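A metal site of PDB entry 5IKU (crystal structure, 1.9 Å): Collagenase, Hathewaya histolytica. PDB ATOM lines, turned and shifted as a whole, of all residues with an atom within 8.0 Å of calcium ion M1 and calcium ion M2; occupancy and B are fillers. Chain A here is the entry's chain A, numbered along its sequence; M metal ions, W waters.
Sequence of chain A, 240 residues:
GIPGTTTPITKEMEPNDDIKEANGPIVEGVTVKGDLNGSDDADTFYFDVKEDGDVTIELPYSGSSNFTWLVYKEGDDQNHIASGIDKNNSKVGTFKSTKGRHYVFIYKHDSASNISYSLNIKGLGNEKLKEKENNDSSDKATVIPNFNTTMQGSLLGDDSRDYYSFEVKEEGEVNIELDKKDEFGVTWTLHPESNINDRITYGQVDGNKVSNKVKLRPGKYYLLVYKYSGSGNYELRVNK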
ATOM      1  N   GLU A 131     -21.068 -19.843  -8.380  1.00  0.00           N
ATOM      2  CA  GLU A 131     -20.558 -20.955  -7.565  1.00  0.00           C
ATOM      3  C   GLU A 131     -20.199 -22.110  -8.496  1.00  0.00           C
ATOM      4  O   GLU A 131     -20.642 -22.166  -9.659  1.00  0.00           O
ATOM      5  CB  GLU A 131     -21.636 -21.478  -6.612  1.00  0.00           C
ATOM      6  CG  GLU A 131     -22.880 -21.950  -7.334  1.00  0.00           C
ATOM      7  CD  GLU A 131     -23.832 -22.699  -6.388  1.00  0.00           C
ATOM      8  OE1 GLU A 131     -23.350 -23.397  -5.459  1.00  0.00           O
ATOM      9  OE2 GLU A 131     -25.066 -22.618  -6.591  1.00  0.00           O
ATOM     10  N   LYS A 132     -19.378 -23.008  -7.970  1.00  0.00           N
ATOM     11  CA  LYS A 132     -18.905 -24.170  -8.727  1.00  0.00           C
ATOM     12  C   LYS A 132     -19.317 -25.465  -8.038  1.00  0.00           C
ATOM     13  O   LYS A 132     -18.707 -25.895  -7.060  1.00  0.00           O
ATOM     14  CB  LYS A 132     -17.397 -24.118  -8.873  1.00  0.00           C
ATOM     15  CG  LYS A 132     -16.967 -22.846  -9.585  1.00  0.00           C
ATOM     16  CD  LYS A 132     -15.497 -22.908  -9.965  1.00  0.00           C
ATOM     17  CE  LYS A 132     -15.082 -21.557 -10.553  1.00  0.00           C
ATOM     18  NZ  LYS A 132     -15.617 -21.423 -11.942  1.00  0.00           N
ATOM     19  N   GLU A 133     -20.333 -26.099  -8.558  1.00  0.00           N
ATOM     20  CA  GLU A 133     -20.724 -27.398  -7.999  1.00  0.00           C
ATOM     21  C   GLU A 133     -19.729 -28.462  -8.529  1.00  0.00           C
ATOM     22  O   GLU A 133     -19.123 -28.235  -9.546  1.00  0.00           O
ATOM     23  CB  GLU A 133     -22.160 -27.669  -8.420  1.00  0.00           C
ATOM     24  CG  GLU A 133     -23.106 -26.746  -7.670  1.00  0.00           C
ATOM     25  CD  GLU A 133     -23.378 -27.142  -6.207  1.00  0.00           C
ATOM     26  OE1 GLU A 133     -22.836 -28.140  -5.674  1.00  0.00           O
ATOM     27  OE2 GLU A 133     -24.169 -26.427  -5.557  1.00  0.00           O
ATOM     28  N   ASN A 134     -19.519 -29.586  -7.842  1.00  0.00           N
ATOM     29  CA  ASN A 134     -20.115 -29.905  -6.531  1.00  0.00           C
ATOM     30  C   ASN A 134     -19.357 -29.168  -5.423  1.00  0.00           C
ATOM     31  O   ASN A 134     -18.149 -29.263  -5.367  1.00  0.00           O
ATOM     32  CB  ASN A 134     -19.904 -31.421  -6.338  1.00  0.00           C
ATOM     33  CG  ASN A 134     -20.701 -31.995  -5.189  1.00  0.00           C
ATOM     34  OD1 ASN A 134     -20.701 -31.505  -4.077  1.00  0.00           O
ATOM     35  ND2 ASN A 134     -21.364 -33.093  -5.466  1.00  0.00           N
ATOM     36  N   ASN A 135     -20.042 -28.451  -4.527  1.00  0.00           N
ATOM     37  CA  ASN A 135     -19.328 -27.788  -3.431  1.00  0.00           C
ATOM     38  C   ASN A 135     -19.955 -28.170  -2.091  1.00  0.00           C
ATOM     39  O   ASN A 135     -19.965 -27.372  -1.152  1.00  0.00           O
ATOM     40  CB  ASN A 135     -19.335 -26.237  -3.607  1.00  0.00           C
ATOM     41  CG  ASN A 135     -20.718 -25.678  -3.888  1.00  0.00           C
ATOM     42  OD1 ASN A 135     -21.738 -26.337  -3.653  1.00  0.00           O
ATOM     43  ND2 ASN A 135     -20.762 -24.432  -4.400  1.00  0.00           N
ATOM     44  N   ASP A 136     -20.459 -29.406  -2.012  1.00  0.00           N
ATOM     45  CA  ASP A 136     -21.221 -29.846  -0.844  1.00  0.00           C
ATOM     46  C   ASP A 136     -20.394 -30.205   0.398  1.00  0.00           C
ATOM     47  O   ASP A 136     -20.969 -30.489   1.444  1.00  0.00           O
ATOM     48  CB  ASP A 136     -22.103 -31.058  -1.195  1.00  0.00           C
ATOM     49  CG  ASP A 136     -23.088 -30.753  -2.333  1.00  0.00           C
ATOM     50  OD1 ASP A 136     -23.700 -31.712  -2.826  1.00  0.00           O
ATOM     51  OD2 ASP A 136     -23.256 -29.585  -2.717  1.00  0.00           O
ATOM     52  N   SER A 137     -19.062 -30.196   0.310  1.00  0.00           N
ATOM     53  CA  SER A 137     -18.240 -30.412   1.489  1.00  0.00           C
ATOM     54  C   SER A 137     -17.092 -29.398   1.479  1.00  0.00           C
ATOM     55  O   SER A 137     -16.788 -28.796   0.440  1.00  0.00           O
ATOM     56  CB  SER A 137     -17.731 -31.858   1.528  1.00  0.00           C
ATOM     57  OG  SER A 137     -17.080 -32.132   0.304  1.00  0.00           O
ATOM     58  N   LYS A 140     -14.410 -29.261  -1.141  1.00  0.00           N
ATOM     59  CA  LYS A 140     -14.818 -28.875  -2.495  1.00  0.00           C
ATOM     60  C   LYS A 140     -15.367 -27.417  -2.516  1.00  0.00           C
ATOM     61  O   LYS A 140     -16.129 -27.047  -3.405  1.00  0.00           O
ATOM     62  CB  LYS A 140     -15.799 -29.916  -3.074  1.00  0.00           C
ATOM     63  CG  LYS A 140     -15.154 -31.261  -3.459  1.00  0.00           C
ATOM     64  CD  LYS A 140     -16.105 -32.340  -3.971  1.00  0.00           C
ATOM     65  CE  LYS A 140     -16.476 -33.404  -2.944  1.00  0.00           C
ATOM     66  NZ  LYS A 140     -17.583 -32.963  -2.051  1.00  0.00           N
ATOM     67  N   THR A 142     -16.188 -23.543  -2.980  1.00  0.00           N
ATOM     68  CA  THR A 142     -15.938 -22.621  -4.061  1.00  0.00           C
ATOM     69  C   THR A 142     -15.164 -21.433  -3.475  1.00  0.00           C
ATOM     70  O   THR A 142     -15.600 -20.828  -2.506  1.00  0.00           O
ATOM     71  CB  THR A 142     -17.283 -22.101  -4.598  1.00  0.00           C
ATOM     72  OG1 THR A 142     -17.996 -23.216  -5.124  1.00  0.00           O
ATOM     73  CG2 THR A 142     -17.054 -20.950  -5.648  1.00  0.00           C
ATOM     74  N   GLN A 152     -22.948 -15.747  -7.275  1.00  0.00           N
ATOM     75  CA  GLN A 152     -24.335 -16.076  -7.586  1.00  0.00           C
ATOM     76  C   GLN A 152     -24.519 -17.579  -7.346  1.00  0.00           C
ATOM     77  O   GLN A 152     -23.788 -18.377  -7.905  1.00  0.00           O
ATOM     78  CB  GLN A 152     -24.613 -15.758  -9.062  1.00  0.00           C
ATOM     79  CG  GLN A 152     -24.450 -14.278  -9.377  1.00  0.00           C
ATOM     80  CD  GLN A 152     -24.571 -13.935 -10.853  1.00  0.00           C
ATOM     81  OE1 GLN A 152     -23.899 -14.510 -11.742  1.00  0.00           O
ATOM     82  NE2 GLN A 152     -25.421 -12.961 -11.141  1.00  0.00           N
ATOM     83  N   GLY A 153     -25.491 -17.965  -6.511  1.00  0.00           N
ATOM     84  CA  GLY A 153     -25.684 -19.373  -6.277  1.00  0.00           C
ATOM     85  C   GLY A 153     -27.136 -19.762  -6.214  1.00  0.00           C
ATOM     86  O   GLY A 153     -28.014 -18.913  -6.213  1.00  0.00           O
ATOM     87  N   SER A 154     -27.392 -21.069  -6.172  1.00  0.00           N
ATOM     88  CA  SER A 154     -28.755 -21.561  -5.938  1.00  0.00           C
ATOM     89  C   SER A 154     -28.659 -22.831  -5.100  1.00  0.00           C
ATOM     90  O   SER A 154     -27.608 -23.516  -5.073  1.00  0.00           O
ATOM     91  CB  SER A 154     -29.495 -21.896  -7.241  1.00  0.00           C
ATOM     92  OG  SER A 154     -28.775 -22.904  -7.914  1.00  0.00           O
ATOM     93  N   LEU A 155     -29.777 -23.116  -4.448  1.00  0.00           N
ATOM     94  CA  LEU A 155     -29.988 -24.300  -3.611  1.00  0.00           C
ATOM     95  C   LEU A 155     -31.365 -24.853  -4.015  1.00  0.00           C
ATOM     96  O   LEU A 155     -32.360 -24.688  -3.289  1.00  0.00           O
ATOM     97  CB  LEU A 155     -30.009 -23.884  -2.135  1.00  0.00           C
ATOM     98  CG  LEU A 155     -28.679 -23.402  -1.565  1.00  0.00           C
ATOM     99  CD1 LEU A 155     -28.906 -22.630  -0.273  1.00  0.00           C
ATOM    100  CD2 LEU A 155     -27.766 -24.611  -1.350  1.00  0.00           C
ATOM    101  N   LEU A 156     -31.418 -25.464  -5.191  1.00  0.00           N
ATOM    102  CA  LEU A 156     -32.683 -25.993  -5.721  1.00  0.00           C
ATOM    103  C   LEU A 156     -32.713 -27.504  -5.476  1.00  0.00           C
ATOM    104  O   LEU A 156     -31.690 -28.166  -5.609  1.00  0.00           O
ATOM    105  CB  LEU A 156     -32.819 -25.657  -7.215  1.00  0.00           C
ATOM    106  CG  LEU A 156     -32.575 -24.178  -7.573  1.00  0.00           C
ATOM    107  CD1 LEU A 156     -32.384 -24.041  -9.067  1.00  0.00           C
ATOM    108  CD2 LEU A 156     -33.711 -23.301  -7.089  1.00  0.00           C
ATOM    109  N   ASP A 158     -32.276 -31.133  -4.559  1.00  0.00           N
ATOM    110  CA  ASP A 158     -31.340 -32.002  -3.839  1.00  0.00           C
ATOM    111  C   ASP A 158     -30.233 -31.201  -3.181  1.00  0.00           C
ATOM    112  O   ASP A 158     -29.696 -31.627  -2.163  1.00  0.00           O
ATOM    113  CB  ASP A 158     -30.663 -32.972  -4.805  1.00  0.00           C
ATOM    114  CG  ASP A 158     -31.570 -34.071  -5.230  1.00  0.00           C
ATOM    115  OD1 ASP A 158     -32.766 -33.826  -5.484  1.00  0.00           O
ATOM    116  OD2 ASP A 158     -31.069 -35.207  -5.331  1.00  0.00           O
ATOM    117  N   ASP A 159     -29.903 -30.062  -3.789  1.00  0.00           N
ATOM    118  CA  ASP A 159     -28.781 -29.230  -3.382  1.00  0.00           C
ATOM    119  C   ASP A 159     -29.159 -28.384  -2.178  1.00  0.00           C
ATOM    120  O   ASP A 159     -29.950 -27.438  -2.308  1.00  0.00           O
ATOM    121  CB  ASP A 159     -28.402 -28.311  -4.559  1.00  0.00           C
ATOM    122  CG  ASP A 159     -27.125 -27.532  -4.325  1.00  0.00           C
ATOM    123  OD1 ASP A 159     -26.144 -28.061  -3.759  1.00  0.00           O
ATOM    124  OD2 ASP A 159     -27.104 -26.357  -4.748  1.00  0.00           O
ATOM    125  N   SER A 160     -28.582 -28.710  -1.019  1.00  0.00           N
ATOM    126  CA  SER A 160     -28.921 -28.032   0.239  1.00  0.00           C
ATOM    127  C   SER A 160     -27.745 -27.377   0.955  1.00  0.00           C
ATOM    128  O   SER A 160     -27.952 -26.633   1.913  1.00  0.00           O
ATOM    129  CB  SER A 160     -29.614 -29.026   1.211  1.00  0.00           C
ATOM    130  OG  SER A 160     -28.640 -29.970   1.655  1.00  0.00           O
ATOM    131  N   ARG A 161     -26.515 -27.625   0.492  1.00  0.00           N
ATOM    132  CA  ARG A 161     -25.340 -26.984   1.073  1.00  0.00           C
ATOM    133  C   ARG A 161     -24.442 -26.466  -0.031  1.00  0.00           C
ATOM    134  O   ARG A 161     -24.183 -27.186  -0.981  1.00  0.00           O
ATOM    135  CB  ARG A 161     -24.495 -27.986   1.829  1.00  0.00           C
ATOM    136  CG  ARG A 161     -25.290 -28.733   2.890  1.00  0.00           C
ATOM    137  CD  ARG A 161     -24.817 -30.174   3.011  1.00  0.00           C
ATOM    138  NE  ARG A 161     -23.806 -30.309   4.037  1.00  0.00           N
ATOM    139  CZ  ARG A 161     -24.063 -30.316   5.347  1.00  0.00           C
ATOM    140  NH1 ARG A 161     -25.295 -30.181   5.806  1.00  0.00           N
ATOM    141  NH2 ARG A 161     -23.066 -30.466   6.199  1.00  0.00           N
ATOM    142  N   ASP A 162     -23.943 -25.243   0.120  1.00  0.00           N
ATOM    143  CA  ASP A 162     -22.912 -24.709  -0.778  1.00  0.00           C
ATOM    144  C   ASP A 162     -21.840 -24.197   0.153  1.00  0.00           C
ATOM    145  O   ASP A 162     -22.083 -23.275   0.949  1.00  0.00           O
ATOM    146  CB  ASP A 162     -23.424 -23.507  -1.581  1.00  0.00           C
ATOM    147  CG  ASP A 162     -24.489 -23.879  -2.601  1.00  0.00           C
ATOM    148  OD1 ASP A 162     -24.548 -25.036  -3.029  1.00  0.00           O
ATOM    149  OD2 ASP A 162     -25.287 -23.011  -3.012  1.00  0.00           O
ATOM    150  N   TYR A 163     -20.643 -24.775   0.072  1.00  0.00           N
ATOM    151  CA  TYR A 163     -19.522 -24.261   0.864  1.00  0.00           C
ATOM    152  C   TYR A 163     -18.691 -23.329   0.009  1.00  0.00           C
ATOM    153  O   TYR A 163     -18.447 -23.599  -1.177  1.00  0.00           O
ATOM    154  CB  TYR A 163     -18.567 -25.389   1.215  1.00  0.00           C
ATOM    155  CG  TYR A 163     -18.897 -26.138   2.470  1.00  0.00           C
ATOM    156  CD1 TYR A 163     -19.672 -27.292   2.431  1.00  0.00           C
ATOM    157  CD2 TYR A 163     -18.420 -25.699   3.691  1.00  0.00           C
ATOM    158  CE1 TYR A 163     -19.970 -27.990   3.587  1.00  0.00           C
ATOM    159  CE2 TYR A 163     -18.684 -26.396   4.856  1.00  0.00           C
ATOM    160  CZ  TYR A 163     -19.471 -27.524   4.796  1.00  0.00           C
ATOM    161  OH  TYR A 163     -19.727 -28.199   5.963  1.00  0.00           O
ATOM    162  N   TYR A 164     -18.240 -22.253   0.628  1.00  0.00           N
ATOM    163  CA  TYR A 164     -17.371 -21.279  -0.032  1.00  0.00           C
ATOM    164  C   TYR A 164     -16.158 -21.146   0.882  1.00  0.00           C
ATOM    165  O   TYR A 164     -16.266 -21.446   2.061  1.00  0.00           O
ATOM    166  CB  TYR A 164     -18.096 -19.913  -0.117  1.00  0.00           C
ATOM    167  CG  TYR A 164     -19.253 -19.879  -1.090  1.00  0.00           C
ATOM    168  CD1 TYR A 164     -20.552 -20.242  -0.662  1.00  0.00           C
ATOM    169  CD2 TYR A 164     -19.076 -19.505  -2.432  1.00  0.00           C
ATOM    170  CE1 TYR A 164     -21.612 -20.205  -1.539  1.00  0.00           C
ATOM    171  CE2 TYR A 164     -20.145 -19.470  -3.306  1.00  0.00           C
ATOM    172  CZ  TYR A 164     -21.411 -19.812  -2.831  1.00  0.00           C
ATOM    173  OH  TYR A 164     -22.487 -19.797  -3.674  1.00  0.00           O
ATOM    174  N   LEU A 224     -20.454 -21.882   5.074  1.00  0.00           N
ATOM    175  CA  LEU A 224     -21.442 -22.835   4.585  1.00  0.00           C
ATOM    176  C   LEU A 224     -22.819 -22.153   4.387  1.00  0.00           C
ATOM    177  O   LEU A 224     -23.392 -21.640   5.343  1.00  0.00           O
ATOM    178  CB  LEU A 224     -21.567 -24.012   5.577  1.00  0.00           C
ATOM    179  CG  LEU A 224     -22.813 -24.897   5.503  1.00  0.00           C
ATOM    180  CD1 LEU A 224     -22.877 -25.622   4.171  1.00  0.00           C
ATOM    181  CD2 LEU A 224     -22.851 -25.905   6.624  1.00  0.00           C
ATOM    182  N   VAL A 225     -23.349 -22.138   3.166  1.00  0.00           N
ATOM    183  CA  VAL A 225     -24.680 -21.581   2.908  1.00  0.00           C
ATOM    184  C   VAL A 225     -25.545 -22.818   2.841  1.00  0.00           C
ATOM    185  O   VAL A 225     -25.246 -23.753   2.109  1.00  0.00           O
ATOM    186  CB  VAL A 225     -24.738 -20.802   1.570  1.00  0.00           C
ATOM    187  CG1 VAL A 225     -26.140 -20.271   1.312  1.00  0.00           C
ATOM    188  CG2 VAL A 225     -23.732 -19.653   1.594  1.00  0.00           C
ATOM    189  N   GLY A 232     -34.352 -21.976  -3.671  1.00  0.00           N
ATOM    190  CA  GLY A 232     -34.248 -20.667  -4.248  1.00  0.00           C
ATOM    191  C   GLY A 232     -32.811 -20.307  -4.620  1.00  0.00           C
ATOM    192  O   GLY A 232     -31.884 -21.104  -4.418  1.00  0.00           O
ATOM    193  N   TYR A 234     -29.710 -17.092  -4.562  1.00  0.00           N
ATOM    194  CA  TYR A 234     -29.215 -16.062  -3.653  1.00  0.00           C
ATOM    195  C   TYR A 234     -27.973 -15.436  -4.291  1.00  0.00           C
ATOM    196  O   TYR A 234     -27.410 -15.977  -5.261  1.00  0.00           O
ATOM    197  CB  TYR A 234     -28.858 -16.711  -2.312  1.00  0.00           C
ATOM    198  CG  TYR A 234     -27.768 -17.765  -2.402  1.00  0.00           C
ATOM    199  CD1 TYR A 234     -28.084 -19.117  -2.590  1.00  0.00           C
ATOM    200  CD2 TYR A 234     -26.424 -17.413  -2.332  1.00  0.00           C
ATOM    201  CE1 TYR A 234     -27.090 -20.065  -2.683  1.00  0.00           C
ATOM    202  CE2 TYR A 234     -25.433 -18.368  -2.437  1.00  0.00           C
ATOM    203  CZ  TYR A 234     -25.774 -19.693  -2.620  1.00  0.00           C
ATOM    204  OH  TYR A 234     -24.773 -20.610  -2.708  1.00  0.00           O
HETATM  205 CA    CA M   1     -25.624 -24.558  -5.179  1.00  0.00          CA
HETATM  206 CA    CA M   2     -23.874 -27.335  -3.352  1.00  0.00          CA
HETATM  207  O   HOH W   1     -26.156 -25.217  -7.524  1.00  0.00           O
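The nearest printed residue that does not touch calcium ion M2 is Glu 131 (4.5 Å).
Calcium ion M1 is bound by O of Ser 154, OD2 of Asp 159, OE2 of Glu 133, OD1 of Asp 162, OE2 of Glu 131, water W1, OE1 of Glu 131 and OD2 of Asp 162. Calcium ion M1 has eight donor atoms within binding distance.
Within 4 Å of calcium ion M1: Glu 131, Glu 133, Ser 154, Asp 159 and Asp 162. The nearest printed residue that does not touch calcium ion M1 is Leu 155 (4.4 Å).
N of Val 225 lies within hydrogen-bond range of O of Asp 162, at 2.8 Å. The side-chain amide oxygen (OD1) of Asn 134 is in hydrogen-bond range of the backbone NH (N) of Asp 136. O of Gln 152 sits at hydrogen-bond distance from N of Glu 131 (3.1 Å). The side-chain carboxylate of Glu 131 sits close to the side-chain amide nitrogen of Asn 135, at 3.0 Å. The side-chain carboxylate (OD2) of Asp 162 lies close to the side-chain hydroxyl (OH) of Tyr 234, at 2.5 Å. N of Tyr 163 sits at hydrogen-bond distance from O of Asn 135. The side-chain amide nitrogen of Asn 135 is in hydrogen-bond range of the side-chain hydroxyl of Thr 142.
OD1 of Asn 135 binds calcium ion M2 (2.4 Å). The backbone carbonyl oxygen (O) of Arg 161 binds calcium ion M2. Calcium ion M2 is bound by the side-chain carboxylate (OE2) of Glu 133 (2.4 Å). OD1 of Asp 162 is bound to calcium ion M2 (2.4 Å). Calcium ion M2 is bound by OD1 of Asp 159. Calcium ion M2 is bound by OD2 of Asp 136. Calcium ion M2 is bound by OE1 of Glu 133, at 2.7 Å.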
